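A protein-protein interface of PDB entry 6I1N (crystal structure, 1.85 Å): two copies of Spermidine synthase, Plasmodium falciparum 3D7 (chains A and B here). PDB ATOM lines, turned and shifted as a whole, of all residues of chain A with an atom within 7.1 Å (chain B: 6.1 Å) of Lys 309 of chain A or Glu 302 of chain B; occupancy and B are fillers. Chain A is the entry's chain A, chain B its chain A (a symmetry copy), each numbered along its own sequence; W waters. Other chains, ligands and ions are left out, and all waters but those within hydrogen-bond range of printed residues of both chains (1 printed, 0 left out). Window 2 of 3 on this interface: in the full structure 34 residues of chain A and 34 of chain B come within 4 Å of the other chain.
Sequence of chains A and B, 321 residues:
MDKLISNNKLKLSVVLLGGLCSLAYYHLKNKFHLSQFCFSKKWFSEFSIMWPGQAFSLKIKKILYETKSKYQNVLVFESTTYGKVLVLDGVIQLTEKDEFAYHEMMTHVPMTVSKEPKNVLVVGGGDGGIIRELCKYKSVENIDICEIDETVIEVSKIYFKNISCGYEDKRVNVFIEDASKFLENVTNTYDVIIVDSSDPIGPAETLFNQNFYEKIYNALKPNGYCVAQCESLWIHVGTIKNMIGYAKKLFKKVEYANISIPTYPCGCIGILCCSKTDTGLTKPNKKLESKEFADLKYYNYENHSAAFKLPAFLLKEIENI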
ATOM      1  N   TYR A 256     -31.964   9.033 -24.653  1.00  0.00           N
ATOM      2  CA  TYR A 256     -31.231  10.147 -24.061  1.00  0.00           C
ATOM      3  C   TYR A 256     -29.805  10.147 -24.585  1.00  0.00           C
ATOM      4  O   TYR A 256     -29.126   9.119 -24.543  1.00  0.00           O
ATOM      5  CB  TYR A 256     -31.250  10.065 -22.541  1.00  0.00           C
ATOM      6  CG  TYR A 256     -30.618  11.258 -21.824  1.00  0.00           C
ATOM      7  CD1 TYR A 256     -29.263  11.264 -21.487  1.00  0.00           C
ATOM      8  CD2 TYR A 256     -31.389  12.358 -21.448  1.00  0.00           C
ATOM      9  CE1 TYR A 256     -28.692  12.354 -20.792  1.00  0.00           C
ATOM     10  CE2 TYR A 256     -30.833  13.438 -20.767  1.00  0.00           C
ATOM     11  CZ  TYR A 256     -29.484  13.427 -20.447  1.00  0.00           C
ATOM     12  OH  TYR A 256     -28.933  14.500 -19.796  1.00  0.00           O
ATOM     13  N   ALA A 257     -29.369  11.278 -25.125  1.00  0.00           N
ATOM     14  CA  ALA A 257     -28.009  11.437 -25.620  1.00  0.00           C
ATOM     15  C   ALA A 257     -27.322  12.565 -24.867  1.00  0.00           C
ATOM     16  O   ALA A 257     -27.981  13.459 -24.319  1.00  0.00           O
ATOM     17  CB  ALA A 257     -27.965  11.726 -27.128  1.00  0.00           C
ATOM     18  N   ASN A 258     -25.985  12.527 -24.883  1.00  0.00           N
ATOM     19  CA  ASN A 258     -25.153  13.490 -24.172  1.00  0.00           C
ATOM     20  C   ASN A 258     -24.290  14.276 -25.153  1.00  0.00           C
ATOM     21  O   ASN A 258     -23.728  13.708 -26.089  1.00  0.00           O
ATOM     22  CB  ASN A 258     -24.254  12.794 -23.143  1.00  0.00           C
ATOM     23  CG  ASN A 258     -23.599  13.790 -22.187  1.00  0.00           C
ATOM     24  OD1 ASN A 258     -24.242  14.738 -21.729  1.00  0.00           O
ATOM     25  ND2 ASN A 258     -22.324  13.574 -21.882  1.00  0.00           N
ATOM     26  N   THR A 282     -31.157   6.710 -32.525  1.00  0.00           N
ATOM     27  CA  THR A 282     -29.730   6.458 -32.321  1.00  0.00           C
ATOM     28  C   THR A 282     -28.955   6.240 -33.618  1.00  0.00           C
ATOM     29  O   THR A 282     -27.724   6.375 -33.622  1.00  0.00           O
ATOM     30  CB  THR A 282     -29.520   5.235 -31.414  1.00  0.00           C
ATOM     31  OG1 THR A 282     -29.969   4.059 -32.101  1.00  0.00           O
ATOM     32  CG2 THR A 282     -30.303   5.374 -30.121  1.00  0.00           C
ATOM     33  N   HIS A 304     -23.002  10.584 -33.806  1.00  0.00           N
ATOM     34  CA  HIS A 304     -24.434  10.468 -33.628  1.00  0.00           C
ATOM     35  C   HIS A 304     -24.755   9.303 -32.702  1.00  0.00           C
ATOM     36  O   HIS A 304     -25.388   9.473 -31.658  1.00  0.00           O
ATOM     37  CB  HIS A 304     -25.065  10.298 -35.039  1.00  0.00           C
ATOM     38  CG  HIS A 304     -26.558  10.196 -35.050  1.00  0.00           C
ATOM     39  ND1 HIS A 304     -27.341  10.850 -35.983  1.00  0.00           N
ATOM     40  CD2 HIS A 304     -27.414   9.523 -34.242  1.00  0.00           C
ATOM     41  CE1 HIS A 304     -28.615  10.581 -35.741  1.00  0.00           C
ATOM     42  NE2 HIS A 304     -28.688   9.773 -34.694  1.00  0.00           N
ATOM     43  N   SER A 305     -24.348   8.080 -33.097  1.00  0.00           N
ATOM     44  CA  SER A 305     -24.642   6.902 -32.285  1.00  0.00           C
ATOM     45  C   SER A 305     -23.908   6.947 -30.949  1.00  0.00           C
ATOM     46  O   SER A 305     -24.455   6.528 -29.924  1.00  0.00           O
ATOM     47  CB  SER A 305     -24.269   5.618 -33.053  1.00  0.00           C
ATOM     48  OG  SER A 305     -24.901   5.652 -34.328  1.00  0.00           O
ATOM     49  N   ALA A 306     -22.674   7.444 -30.946  1.00  0.00           N
ATOM     50  CA  ALA A 306     -21.866   7.383 -29.723  1.00  0.00           C
ATOM     51  C   ALA A 306     -22.481   8.213 -28.602  1.00  0.00           C
ATOM     52  O   ALA A 306     -22.282   7.911 -27.409  1.00  0.00           O
ATOM     53  CB  ALA A 306     -20.443   7.863 -30.017  1.00  0.00           C
ATOM     54  N   ALA A 307     -23.260   9.244 -28.962  1.00  0.00           N
ATOM     55  CA  ALA A 307     -23.781  10.174 -27.964  1.00  0.00           C
ATOM     56  C   ALA A 307     -24.828   9.500 -27.101  1.00  0.00           C
ATOM     57  O   ALA A 307     -25.110   9.963 -25.995  1.00  0.00           O
ATOM     58  CB  ALA A 307     -24.369  11.406 -28.658  1.00  0.00           C
ATOM     59  N   PHE A 308     -25.353   8.371 -27.554  1.00  0.00           N
ATOM     60  CA  PHE A 308     -26.343   7.619 -26.796  1.00  0.00           C
ATOM     61  C   PHE A 308     -25.724   6.572 -25.874  1.00  0.00           C
ATOM     62  O   PHE A 308     -26.465   5.916 -25.144  1.00  0.00           O
ATOM     63  CB  PHE A 308     -27.326   6.939 -27.769  1.00  0.00           C
ATOM     64  CG  PHE A 308     -28.208   7.935 -28.518  1.00  0.00           C
ATOM     65  CD1 PHE A 308     -27.742   8.566 -29.663  1.00  0.00           C
ATOM     66  CD2 PHE A 308     -29.470   8.270 -28.029  1.00  0.00           C
ATOM     67  CE1 PHE A 308     -28.554   9.501 -30.352  1.00  0.00           C
ATOM     68  CE2 PHE A 308     -30.289   9.220 -28.722  1.00  0.00           C
ATOM     69  CZ  PHE A 308     -29.821   9.818 -29.860  1.00  0.00           C
ATOM     70  N   LYS A 309     -24.404   6.429 -25.862  1.00  0.00           N
ATOM     71  CA  LYS A 309     -23.724   5.459 -24.984  1.00  0.00           C
ATOM     72  C   LYS A 309     -23.394   6.154 -23.670  1.00  0.00           C
ATOM     73  O   LYS A 309     -22.386   6.843 -23.571  1.00  0.00           O
ATOM     74  CB  LYS A 309     -22.466   4.933 -25.662  1.00  0.00           C
ATOM     75  CG  LYS A 309     -22.701   4.423 -27.091  1.00  0.00           C
ATOM     76  CD  LYS A 309     -23.744   3.329 -27.084  1.00  0.00           C
ATOM     77  CE  LYS A 309     -23.914   2.705 -28.473  1.00  0.00           C
ATOM     78  NZ  LYS A 309     -24.865   1.557 -28.394  1.00  0.00           N
ATOM     79  N   LEU A 310     -24.264   5.986 -22.656  1.00  0.00           N
ATOM     80  CA  LEU A 310     -24.270   6.779 -21.438  1.00  0.00           C
ATOM     81  C   LEU A 310     -23.454   6.100 -20.337  1.00  0.00           C
ATOM     82  O   LEU A 310     -23.257   4.887 -20.350  1.00  0.00           O
ATOM     83  CB  LEU A 310     -25.705   6.973 -20.954  1.00  0.00           C
ATOM     84  CG  LEU A 310     -26.640   7.540 -22.036  1.00  0.00           C
ATOM     85  CD1 LEU A 310     -28.085   7.349 -21.653  1.00  0.00           C
ATOM     86  CD2 LEU A 310     -26.313   8.989 -22.188  1.00  0.00           C
ATOM     87  N   PRO A 311     -22.972   6.863 -19.366  1.00  0.00           N
ATOM     88  CA  PRO A 311     -22.285   6.246 -18.211  1.00  0.00           C
ATOM     89  C   PRO A 311     -23.175   5.274 -17.445  1.00  0.00           C
ATOM     90  O   PRO A 311     -24.390   5.460 -17.324  1.00  0.00           O
ATOM     91  CB  PRO A 311     -21.911   7.456 -17.332  1.00  0.00           C
ATOM     92  CG  PRO A 311     -21.819   8.600 -18.281  1.00  0.00           C
ATOM     93  CD  PRO A 311     -22.897   8.340 -19.342  1.00  0.00           C
ATOM     94  N   LEU A 315     -27.615   4.870 -16.944  1.00  0.00           N
ATOM     95  CA  LEU A 315     -28.333   3.686 -17.415  1.00  0.00           C
ATOM     96  C   LEU A 315     -29.071   2.980 -16.290  1.00  0.00           C
ATOM     97  O   LEU A 315     -30.213   2.554 -16.461  1.00  0.00           O
ATOM     98  CB  LEU A 315     -27.364   2.711 -18.049  1.00  0.00           C
ATOM     99  CG  LEU A 315     -26.759   3.161 -19.355  1.00  0.00           C
ATOM    100  CD1 LEU A 315     -25.993   1.973 -19.935  1.00  0.00           C
ATOM    101  CD2 LEU A 315     -27.871   3.621 -20.313  1.00  0.00           C
ATOM    102  N   ASN B 300     -18.528   0.970 -19.221  1.00  0.00           N
ATOM    103  CA  ASN B 300     -19.086  -0.320 -19.636  1.00  0.00           C
ATOM    104  C   ASN B 300     -18.598  -0.662 -21.039  1.00  0.00           C
ATOM    105  O   ASN B 300     -17.916   0.122 -21.703  1.00  0.00           O
ATOM    106  CB  ASN B 300     -20.631  -0.364 -19.548  1.00  0.00           C
ATOM    107  CG  ASN B 300     -21.329   0.691 -20.426  1.00  0.00           C
ATOM    108  OD1 ASN B 300     -20.891   1.012 -21.533  1.00  0.00           O
ATOM    109  ND2 ASN B 300     -22.427   1.224 -19.913  1.00  0.00           N
ATOM    110  N   TYR B 301     -18.933  -1.885 -21.472  1.00  0.00           N
ATOM    111  CA  TYR B 301     -18.454  -2.397 -22.755  1.00  0.00           C
ATOM    112  C   TYR B 301     -18.743  -1.431 -23.914  1.00  0.00           C
ATOM    113  O   TYR B 301     -17.870  -1.157 -24.752  1.00  0.00           O
ATOM    114  CB  TYR B 301     -19.097  -3.769 -22.998  1.00  0.00           C
ATOM    115  CG  TYR B 301     -18.650  -4.490 -24.245  1.00  0.00           C
ATOM    116  CD1 TYR B 301     -17.561  -5.348 -24.216  1.00  0.00           C
ATOM    117  CD2 TYR B 301     -19.338  -4.335 -25.453  1.00  0.00           C
ATOM    118  CE1 TYR B 301     -17.154  -6.036 -25.355  1.00  0.00           C
ATOM    119  CE2 TYR B 301     -18.937  -5.015 -26.595  1.00  0.00           C
ATOM    120  CZ  TYR B 301     -17.841  -5.860 -26.537  1.00  0.00           C
ATOM    121  OH  TYR B 301     -17.424  -6.537 -27.661  1.00  0.00           O
ATOM    122  N   GLU B 302     -19.944  -0.867 -23.950  1.00  0.00           N
ATOM    123  CA  GLU B 302     -20.283   0.070 -25.025  1.00  0.00           C
ATOM    124  C   GLU B 302     -19.579   1.435 -24.882  1.00  0.00           C
ATOM    125  O   GLU B 302     -19.107   2.003 -25.883  1.00  0.00           O
ATOM    126  CB  GLU B 302     -21.808   0.204 -25.081  1.00  0.00           C
ATOM    127  CG  GLU B 302     -22.463  -1.154 -25.455  1.00  0.00           C
ATOM    128  CD  GLU B 302     -23.797  -1.040 -26.173  1.00  0.00           C
ATOM    129  OE1 GLU B 302     -24.453   0.026 -26.091  1.00  0.00           O
ATOM    130  OE2 GLU B 302     -24.192  -2.039 -26.822  1.00  0.00           O
ATOM    131  N   ASN B 303     -19.451   1.949 -23.648  1.00  0.00           N
ATOM    132  CA  ASN B 303     -18.816   3.251 -23.436  1.00  0.00           C
ATOM    133  C   ASN B 303     -17.375   3.250 -23.876  1.00  0.00           C
ATOM    134  O   ASN B 303     -16.862   4.273 -24.338  1.00  0.00           O
ATOM    135  CB  ASN B 303     -18.882   3.626 -21.958  1.00  0.00           C
ATOM    136  CG  ASN B 303     -20.277   3.878 -21.534  1.00  0.00           C
ATOM    137  OD1 ASN B 303     -21.182   4.002 -22.396  1.00  0.00           O
ATOM    138  ND2 ASN B 303     -20.501   3.927 -20.230  1.00  0.00           N
ATOM    139  N   HIS B 304     -16.706   2.114 -23.687  1.00  0.00           N
ATOM    140  CA  HIS B 304     -15.318   1.952 -24.070  1.00  0.00           C
ATOM    141  C   HIS B 304     -15.108   2.433 -25.499  1.00  0.00           C
ATOM    142  O   HIS B 304     -14.301   3.329 -25.760  1.00  0.00           O
ATOM    143  CB  HIS B 304     -14.958   0.449 -23.889  1.00  0.00           C
ATOM    144  CG  HIS B 304     -13.539   0.101 -24.210  1.00  0.00           C
ATOM    145  ND1 HIS B 304     -12.789  -0.757 -23.428  1.00  0.00           N
ATOM    146  CD2 HIS B 304     -12.729   0.497 -25.223  1.00  0.00           C
ATOM    147  CE1 HIS B 304     -11.578  -0.869 -23.949  1.00  0.00           C
ATOM    148  NE2 HIS B 304     -11.514  -0.124 -25.043  1.00  0.00           N
ATOM    149  N   SER B 305     -15.816   1.809 -26.462  1.00  0.00           N
ATOM    150  CA  SER B 305     -15.652   2.186 -27.864  1.00  0.00           C
ATOM    151  C   SER B 305     -16.149   3.605 -28.124  1.00  0.00           C
ATOM    152  O   SER B 305     -15.550   4.338 -28.918  1.00  0.00           O
ATOM    153  CB  SER B 305     -16.396   1.189 -28.775  1.00  0.00           C
ATOM    154  OG  SER B 305     -15.975  -0.129 -28.445  1.00  0.00           O
ATOM    155  N   ALA B 306     -17.237   4.001 -27.470  1.00  0.00           N
ATOM    156  CA  ALA B 306     -17.844   5.300 -27.782  1.00  0.00           C
ATOM    157  C   ALA B 306     -16.905   6.453 -27.444  1.00  0.00           C
ATOM    158  O   ALA B 306     -16.977   7.531 -28.066  1.00  0.00           O
ATOM    159  CB  ALA B 306     -19.163   5.451 -27.022  1.00  0.00           C
ATOM    160  N   ALA B 307     -15.994   6.237 -26.483  1.00  0.00           N
ATOM    161  CA  ALA B 307     -15.144   7.322 -26.000  1.00  0.00           C
ATOM    162  C   ALA B 307     -14.140   7.729 -27.059  1.00  0.00           C
ATOM    163  O   ALA B 307     -13.604   8.836 -27.008  1.00  0.00           O
ATOM    164  CB  ALA B 307     -14.427   6.888 -24.718  1.00  0.00           C
HETATM  165  O   HOH W   1     -23.345   2.843 -22.426  1.00  0.00           O
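The side-chain amino group of Lys 309 of chain A lies within salt-bridge range of the side-chain carboxylate of Glu 302 of chain B (2.8 Å).
O of Lys 309 of chain A sits close to OD1 of Asn 303 of chain B.
The side-chain amide nitrogen (ND2) of Asn 303 of chain B is in hydrogen-bond range of the backbone carbonyl oxygen (O) of Leu 310 of chain A, at 2.9 Å.
The side-chain amide oxygen of Asn 300 of chain B is in hydrogen-bond range of the backbone NH of Glu 302 of chain B (3.2 Å).
OD1 of Asn 300 of chain B is in hydrogen-bond range of N of Asn 303 of chain B (2.7 Å).
Among the printed residues, merely in contact across the chains: Pro 311 of chain A with Asn 303 of chain B, Lys 309 of chain A with Ala 306 of chain B, Leu 315 of chain A with Asn 300 of chain B, Leu 310 of chain A with Asn 300 of chain B and Ala 306 of chain A with Ala 306 of chain B.
His 304 of chain A touches none of the printed residues of chain B.
Of the printed residues of chain B, Pro 311 of chain A touches Asn 303 (3.6 Å).
Of the printed residues of chain B, Leu 315 of chain A touches Asn 300 (3.6 Å).
Of chain A, only Lys 309 (2.8 Å) comes within 4 Å of Glu 302 of chain B.
Of the printed residues of chain A, Asn 303 of chain B touches Lys 309, Leu 310 and Pro 311.
The nearest residue of chain B that does not touch Lys 309 of chain A is Asn 300 of chain B (5.9 Å).
Hydrophobic or aromatic side chains of chain B that line the printed part of chain A: Ala 306.
Among the printed residues, Asp or Glu carboxylates within 4 Å of a Lys or Arg side-chain nitrogen of the other chain: Lys 309 of chain A with Glu 302 of chain B (2.8 Å).
Ala 306 of chain A touches its own counterpart, Ala 306 of chain B.
Positions printed for both chains: 304, 305, 306 and 307.
Of the 8 pairs that touch across the chains among the printed residues, 1 has its exchanged pair printed and touching as well.
Water W1 lies within hydrogen-bond range of OD1 of Asn 303 of chain B (2.5 Å), O of Leu 310 of chain A (2.9 Å) and ND2 of Asn 300 of chain B (3.1 Å).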
